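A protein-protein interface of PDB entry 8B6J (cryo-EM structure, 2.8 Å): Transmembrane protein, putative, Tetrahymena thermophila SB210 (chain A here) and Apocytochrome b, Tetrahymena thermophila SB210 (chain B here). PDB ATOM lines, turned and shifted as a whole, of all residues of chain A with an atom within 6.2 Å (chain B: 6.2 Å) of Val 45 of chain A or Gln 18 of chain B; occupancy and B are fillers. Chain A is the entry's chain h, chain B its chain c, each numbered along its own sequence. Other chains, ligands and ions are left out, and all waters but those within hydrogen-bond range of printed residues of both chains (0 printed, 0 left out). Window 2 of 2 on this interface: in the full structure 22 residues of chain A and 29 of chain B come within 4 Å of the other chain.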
ATOM      1  N   VAL A  41     -14.255  -7.248 -17.501  1.00  0.00           N
ATOM      2  CA  VAL A  41     -15.637  -7.543 -17.868  1.00  0.00           C
ATOM      3  C   VAL A  41     -15.682  -8.326 -19.173  1.00  0.00           C
ATOM      4  O   VAL A  41     -16.530  -9.207 -19.358  1.00  0.00           O
ATOM      5  CB  VAL A  41     -16.449  -6.240 -17.960  1.00  0.00           C
ATOM      6  CG1 VAL A  41     -17.782  -6.487 -18.631  1.00  0.00           C
ATOM      7  CG2 VAL A  41     -16.653  -5.652 -16.576  1.00  0.00           C
ATOM      8  N   ASN A  42     -14.778  -8.012 -20.102  1.00  0.00           N
ATOM      9  CA  ASN A  42     -14.746  -8.729 -21.371  1.00  0.00           C
ATOM     10  C   ASN A  42     -14.517 -10.220 -21.166  1.00  0.00           C
ATOM     11  O   ASN A  42     -14.995 -11.036 -21.962  1.00  0.00           O
ATOM     12  CB  ASN A  42     -13.658  -8.144 -22.271  1.00  0.00           C
ATOM     13  CG  ASN A  42     -13.581  -8.834 -23.616  1.00  0.00           C
ATOM     14  OD1 ASN A  42     -14.552  -9.433 -24.076  1.00  0.00           O
ATOM     15  ND2 ASN A  42     -12.420  -8.754 -24.256  1.00  0.00           N
ATOM     16  N   SER A  43     -13.787 -10.598 -20.114  1.00  0.00           N
ATOM     17  CA  SER A  43     -13.537 -12.013 -19.865  1.00  0.00           C
ATOM     18  C   SER A  43     -14.832 -12.762 -19.581  1.00  0.00           C
ATOM     19  O   SER A  43     -15.048 -13.863 -20.101  1.00  0.00           O
ATOM     20  CB  SER A  43     -12.562 -12.178 -18.700  1.00  0.00           C
ATOM     21  OG  SER A  43     -11.319 -11.560 -18.983  1.00  0.00           O
ATOM     22  N   SER A  44     -15.704 -12.187 -18.757  1.00  0.00           N
ATOM     23  CA  SER A  44     -16.936 -12.860 -18.379  1.00  0.00           C
ATOM     24  C   SER A  44     -17.953 -11.837 -17.896  1.00  0.00           C
ATOM     25  O   SER A  44     -17.591 -10.782 -17.370  1.00  0.00           O
ATOM     26  CB  SER A  44     -16.689 -13.902 -17.285  1.00  0.00           C
ATOM     27  OG  SER A  44     -17.883 -14.168 -16.574  1.00  0.00           O
ATOM     28  N   VAL A  45     -19.234 -12.173 -18.080  1.00  0.00           N
ATOM     29  CA  VAL A  45     -20.323 -11.346 -17.563  1.00  0.00           C
ATOM     30  C   VAL A  45     -20.568 -11.565 -16.081  1.00  0.00           C
ATOM     31  O   VAL A  45     -21.410 -10.874 -15.494  1.00  0.00           O
ATOM     32  CB  VAL A  45     -21.638 -11.610 -18.326  1.00  0.00           C
ATOM     33  CG1 VAL A  45     -21.532 -11.102 -19.751  1.00  0.00           C
ATOM     34  CG2 VAL A  45     -21.984 -13.092 -18.314  1.00  0.00           C
ATOM     35  N   ARG A  46     -19.869 -12.511 -15.455  1.00  0.00           N
ATOM     36  CA  ARG A  46     -20.018 -12.744 -14.027  1.00  0.00           C
ATOM     37  C   ARG A  46     -19.335 -11.682 -13.177  1.00  0.00           C
ATOM     38  O   ARG A  46     -19.541 -11.663 -11.960  1.00  0.00           O
ATOM     39  CB  ARG A  46     -19.459 -14.120 -13.657  1.00  0.00           C
ATOM     40  CG  ARG A  46     -20.236 -15.283 -14.238  1.00  0.00           C
ATOM     41  CD  ARG A  46     -19.766 -16.602 -13.653  1.00  0.00           C
ATOM     42  NE  ARG A  46     -20.514 -17.733 -14.187  1.00  0.00           N
ATOM     43  CZ  ARG A  46     -21.669 -18.164 -13.701  1.00  0.00           C
ATOM     44  NH1 ARG A  46     -22.244 -17.582 -12.662  1.00  0.00           N
ATOM     45  NH2 ARG A  46     -22.264 -19.206 -14.274  1.00  0.00           N
ATOM     46  N   TYR A  47     -18.532 -10.807 -13.780  1.00  0.00           N
ATOM     47  CA  TYR A  47     -17.829  -9.782 -13.023  1.00  0.00           C
ATOM     48  C   TYR A  47     -18.708  -8.593 -12.663  1.00  0.00           C
ATOM     49  O   TYR A  47     -18.273  -7.740 -11.883  1.00  0.00           O
ATOM     50  CB  TYR A  47     -16.609  -9.297 -13.808  1.00  0.00           C
ATOM     51  CG  TYR A  47     -15.439 -10.250 -13.747  1.00  0.00           C
ATOM     52  CD1 TYR A  47     -14.622 -10.301 -12.629  1.00  0.00           C
ATOM     53  CD2 TYR A  47     -15.153 -11.098 -14.807  1.00  0.00           C
ATOM     54  CE1 TYR A  47     -13.554 -11.171 -12.567  1.00  0.00           C
ATOM     55  CE2 TYR A  47     -14.086 -11.970 -14.753  1.00  0.00           C
ATOM     56  CZ  TYR A  47     -13.290 -12.002 -13.631  1.00  0.00           C
ATOM     57  OH  TYR A  47     -12.225 -12.869 -13.572  1.00  0.00           O
ATOM     58  N   TYR A  48     -19.924  -8.507 -13.205  1.00  0.00           N
ATOM     59  CA  TYR A  48     -20.828  -7.436 -12.799  1.00  0.00           C
ATOM     60  C   TYR A  48     -21.306  -7.625 -11.366  1.00  0.00           C
ATOM     61  O   TYR A  48     -21.613  -6.643 -10.682  1.00  0.00           O
ATOM     62  CB  TYR A  48     -22.019  -7.364 -13.751  1.00  0.00           C
ATOM     63  CG  TYR A  48     -21.642  -6.965 -15.157  1.00  0.00           C
ATOM     64  CD1 TYR A  48     -21.330  -5.649 -15.464  1.00  0.00           C
ATOM     65  CD2 TYR A  48     -21.600  -7.902 -16.176  1.00  0.00           C
ATOM     66  CE1 TYR A  48     -20.983  -5.281 -16.744  1.00  0.00           C
ATOM     67  CE2 TYR A  48     -21.257  -7.543 -17.459  1.00  0.00           C
ATOM     68  CZ  TYR A  48     -20.949  -6.232 -17.737  1.00  0.00           C
ATOM     69  OH  TYR A  48     -20.609  -5.870 -19.020  1.00  0.00           O
ATOM     70  N   HIS A  49     -21.381  -8.872 -10.899  1.00  0.00           N
ATOM     71  CA  HIS A  49     -21.746  -9.171  -9.515  1.00  0.00           C
ATOM     72  C   HIS A  49     -20.459  -9.219  -8.696  1.00  0.00           C
ATOM     73  O   HIS A  49     -19.879 -10.277  -8.444  1.00  0.00           O
ATOM     74  CB  HIS A  49     -22.520 -10.481  -9.441  1.00  0.00           C
ATOM     75  CG  HIS A  49     -22.994 -10.827  -8.066  1.00  0.00           C
ATOM     76  ND1 HIS A  49     -23.851 -10.020  -7.349  1.00  0.00           N
ATOM     77  CD2 HIS A  49     -22.733 -11.895  -7.276  1.00  0.00           C
ATOM     78  CE1 HIS A  49     -24.096 -10.575  -6.175  1.00  0.00           C
ATOM     79  NE2 HIS A  49     -23.429 -11.714  -6.106  1.00  0.00           N
ATOM     80  N   MET B   9     -22.088  -1.630 -20.302  1.00  0.00           N
ATOM     81  CA  MET B   9     -22.379  -2.934 -20.878  1.00  0.00           C
ATOM     82  C   MET B   9     -22.489  -2.806 -22.387  1.00  0.00           C
ATOM     83  O   MET B   9     -23.046  -1.829 -22.895  1.00  0.00           O
ATOM     84  CB  MET B   9     -23.681  -3.513 -20.313  1.00  0.00           C
ATOM     85  CG  MET B   9     -23.487  -4.682 -19.364  1.00  0.00           C
ATOM     86  SD  MET B   9     -23.148  -6.235 -20.212  1.00  0.00           S
ATOM     87  CE  MET B   9     -24.729  -6.548 -20.991  1.00  0.00           C
ATOM     88  N   ILE B  13     -26.304  -9.407 -28.543  1.00  0.00           N
ATOM     89  CA  ILE B  13     -27.238 -10.501 -28.293  1.00  0.00           C
ATOM     90  C   ILE B  13     -26.569 -11.596 -27.473  1.00  0.00           C
ATOM     91  O   ILE B  13     -27.140 -12.106 -26.503  1.00  0.00           O
ATOM     92  CB  ILE B  13     -27.790 -11.043 -29.623  1.00  0.00           C
ATOM     93  CG1 ILE B  13     -28.683  -9.989 -30.278  1.00  0.00           C
ATOM     94  CG2 ILE B  13     -28.561 -12.332 -29.392  1.00  0.00           C
ATOM     95  CD1 ILE B  13     -28.927 -10.222 -31.743  1.00  0.00           C
ATOM     96  N   LYS B  14     -25.345 -11.970 -27.846  1.00  0.00           N
ATOM     97  CA  LYS B  14     -24.612 -12.973 -27.082  1.00  0.00           C
ATOM     98  C   LYS B  14     -24.460 -12.544 -25.627  1.00  0.00           C
ATOM     99  O   LYS B  14     -24.815 -13.287 -24.702  1.00  0.00           O
ATOM    100  CB  LYS B  14     -23.244 -13.204 -27.729  1.00  0.00           C
ATOM    101  CG  LYS B  14     -22.272 -14.069 -26.936  1.00  0.00           C
ATOM    102  CD  LYS B  14     -22.691 -15.524 -26.900  1.00  0.00           C
ATOM    103  CE  LYS B  14     -21.612 -16.381 -26.262  1.00  0.00           C
ATOM    104  NZ  LYS B  14     -21.960 -17.826 -26.262  1.00  0.00           N
ATOM    105  N   LYS B  15     -23.947 -11.332 -25.409  1.00  0.00           N
ATOM    106  CA  LYS B  15     -23.673 -10.884 -24.048  1.00  0.00           C
ATOM    107  C   LYS B  15     -24.958 -10.618 -23.280  1.00  0.00           C
ATOM    108  O   LYS B  15     -25.022 -10.868 -22.075  1.00  0.00           O
ATOM    109  CB  LYS B  15     -22.786  -9.642 -24.072  1.00  0.00           C
ATOM    110  CG  LYS B  15     -21.327  -9.957 -24.351  1.00  0.00           C
ATOM    111  CD  LYS B  15     -20.466  -8.711 -24.355  1.00  0.00           C
ATOM    112  CE  LYS B  15     -18.988  -9.062 -24.405  1.00  0.00           C
ATOM    113  NZ  LYS B  15     -18.122  -7.849 -24.391  1.00  0.00           N
ATOM    114  N   ILE B  16     -25.996 -10.115 -23.950  1.00  0.00           N
ATOM    115  CA  ILE B  16     -27.272  -9.912 -23.269  1.00  0.00           C
ATOM    116  C   ILE B  16     -27.846 -11.246 -22.812  1.00  0.00           C
ATOM    117  O   ILE B  16     -28.328 -11.378 -21.678  1.00  0.00           O
ATOM    118  CB  ILE B  16     -28.256  -9.159 -24.181  1.00  0.00           C
ATOM    119  CG1 ILE B  16     -27.832  -7.697 -24.319  1.00  0.00           C
ATOM    120  CG2 ILE B  16     -29.671  -9.257 -23.628  1.00  0.00           C
ATOM    121  CD1 ILE B  16     -28.630  -6.929 -25.345  1.00  0.00           C
ATOM    122  N   VAL B  17     -27.813 -12.254 -23.684  1.00  0.00           N
ATOM    123  CA  VAL B  17     -28.333 -13.568 -23.316  1.00  0.00           C
ATOM    124  C   VAL B  17     -27.547 -14.135 -22.142  1.00  0.00           C
ATOM    125  O   VAL B  17     -28.123 -14.652 -21.179  1.00  0.00           O
ATOM    126  CB  VAL B  17     -28.304 -14.516 -24.528  1.00  0.00           C
ATOM    127  CG1 VAL B  17     -28.547 -15.948 -24.089  1.00  0.00           C
ATOM    128  CG2 VAL B  17     -29.344 -14.095 -25.551  1.00  0.00           C
ATOM    129  N   GLN B  18     -26.216 -14.042 -22.199  1.00  0.00           N
ATOM    130  CA  GLN B  18     -25.402 -14.549 -21.098  1.00  0.00           C
ATOM    131  C   GLN B  18     -25.711 -13.812 -19.801  1.00  0.00           C
ATOM    132  O   GLN B  18     -25.874 -14.428 -18.740  1.00  0.00           O
ATOM    133  CB  GLN B  18     -23.919 -14.428 -21.442  1.00  0.00           C
ATOM    134  CG  GLN B  18     -23.428 -15.459 -22.438  1.00  0.00           C
ATOM    135  CD  GLN B  18     -21.920 -15.492 -22.535  1.00  0.00           C
ATOM    136  OE1 GLN B  18     -21.259 -14.459 -22.436  1.00  0.00           O
ATOM    137  NE2 GLN B  18     -21.363 -16.683 -22.717  1.00  0.00           N
ATOM    138  N   TYR B  19     -25.804 -12.483 -19.870  1.00  0.00           N
ATOM    139  CA  TYR B  19     -26.034 -11.682 -18.674  1.00  0.00           C
ATOM    140  C   TYR B  19     -27.376 -12.013 -18.039  1.00  0.00           C
ATOM    141  O   TYR B  19     -27.475 -12.147 -16.815  1.00  0.00           O
ATOM    142  CB  TYR B  19     -25.955 -10.198 -19.037  1.00  0.00           C
ATOM    143  CG  TYR B  19     -26.268  -9.253 -17.904  1.00  0.00           C
ATOM    144  CD1 TYR B  19     -25.310  -8.939 -16.953  1.00  0.00           C
ATOM    145  CD2 TYR B  19     -27.517  -8.662 -17.794  1.00  0.00           C
ATOM    146  CE1 TYR B  19     -25.591  -8.071 -15.919  1.00  0.00           C
ATOM    147  CE2 TYR B  19     -27.807  -7.792 -16.763  1.00  0.00           C
ATOM    148  CZ  TYR B  19     -26.840  -7.500 -15.830  1.00  0.00           C
ATOM    149  OH  TYR B  19     -27.124  -6.634 -14.800  1.00  0.00           O
ATOM    150  N   PHE B  20     -28.422 -12.156 -18.853  1.00  0.00           N
ATOM    151  CA  PHE B  20     -29.740 -12.457 -18.308  1.00  0.00           C
ATOM    152  C   PHE B  20     -29.895 -13.917 -17.907  1.00  0.00           C
ATOM    153  O   PHE B  20     -30.783 -14.230 -17.108  1.00  0.00           O
ATOM    154  CB  PHE B  20     -30.822 -12.072 -19.313  1.00  0.00           C
ATOM    155  CG  PHE B  20     -31.146 -10.609 -19.308  1.00  0.00           C
ATOM    156  CD1 PHE B  20     -30.386  -9.718 -20.040  1.00  0.00           C
ATOM    157  CD2 PHE B  20     -32.201 -10.124 -18.559  1.00  0.00           C
ATOM    158  CE1 PHE B  20     -30.676  -8.372 -20.032  1.00  0.00           C
ATOM    159  CE2 PHE B  20     -32.495  -8.779 -18.549  1.00  0.00           C
ATOM    160  CZ  PHE B  20     -31.730  -7.902 -19.287  1.00  0.00           C
ATOM    161  N   SER B  21     -29.064 -14.815 -18.436  1.00  0.00           N
ATOM    162  CA  SER B  21     -29.083 -16.201 -17.992  1.00  0.00           C
ATOM    163  C   SER B  21     -28.224 -16.438 -16.760  1.00  0.00           C
ATOM    164  O   SER B  21     -28.382 -17.473 -16.104  1.00  0.00           O
ATOM    165  CB  SER B  21     -28.611 -17.124 -19.118  1.00  0.00           C
ATOM    166  OG  SER B  21     -27.283 -16.821 -19.499  1.00  0.00           O
ATOM    167  N   VAL B  22     -27.322 -15.513 -16.433  1.00  0.00           N
ATOM    168  CA  VAL B  22     -26.490 -15.619 -15.239  1.00  0.00           C
ATOM    169  C   VAL B  22     -26.849 -14.577 -14.193  1.00  0.00           C
ATOM    170  O   VAL B  22     -26.174 -14.499 -13.157  1.00  0.00           O
ATOM    171  CB  VAL B  22     -24.994 -15.521 -15.597  1.00  0.00           C
ATOM    172  CG1 VAL B  22     -24.561 -14.067 -15.725  1.00  0.00           C
ATOM    173  CG2 VAL B  22     -24.151 -16.248 -14.569  1.00  0.00           C
ATOM    174  N   MET B  23     -27.886 -13.781 -14.425  1.00  0.00           N
ATOM    175  CA  MET B  23     -28.251 -12.724 -13.494  1.00  0.00           C
ATOM    176  C   MET B  23     -28.751 -13.309 -12.179  1.00  0.00           C
ATOM    177  O   MET B  23     -29.386 -14.367 -12.143  1.00  0.00           O
ATOM    178  CB  MET B  23     -29.332 -11.834 -14.105  1.00  0.00           C
ATOM    179  CG  MET B  23     -29.646 -10.587 -13.305  1.00  0.00           C
ATOM    180  SD  MET B  23     -31.231  -9.874 -13.763  1.00  0.00           S
ATOM    181  CE  MET B  23     -31.011  -9.663 -15.525  1.00  0.00           C
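The side-chain hydroxyl (OG) of Ser 21 of chain B lies within hydrogen-bond range of the backbone carbonyl oxygen (O) of Gln 18 of chain B (2.9 Å). The side-chain hydroxyl (OG) of Ser 44 of chain A lies within hydrogen-bond range of the backbone NH (N) of Arg 46 of chain A (2.8 Å).
The side-chain sulfur (SD) of Met 9 of chain B is in hydrogen-bond range of the side-chain hydroxyl (OH) of Tyr 48 of chain A (2.8 Å).
Of the 9 printed residues of chain A, 4 touch a printed residue of chain B. Among the printed residues, 6 pairs touch across the chains. Among the printed residues, no Asp or Glu carboxylate lies within 4 Å of a Lys or Arg side-chain nitrogen of the other chain.
Val 45 of chain A touches just these residues of chain B: Gln 18 (3.9 Å) and Val 22 (3.8 Å). Gln 18 of chain B touches one residue of chain A. Of the printed residues of chain A, Met 9 of chain B touches Tyr 48 (2.8 Å). Of the printed residues of chain B, Asn 42 of chain A touches Lys 15. Of the printed residues of chain B, Tyr 48 of chain A touches Met 9 (2.8 Å) and Tyr 19 (3.9 Å). Tyr 47 of chain A touches none of the printed residues of chain B. The nearest residue of chain B that does not touch Val 45 of chain A is Tyr 19 of chain B (4.2 Å).
Among the printed residues, pairs that only touch across the chains: Arg 46 of chain A with Val 22 of chain B, Val 45 of chain A with Val 22 of chain B, Val 45 of chain A with Gln 18 of chain B, Asn 42 of chain A with Lys 15 of chain B and Tyr 48 of chain A with Tyr 19 of chain B.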
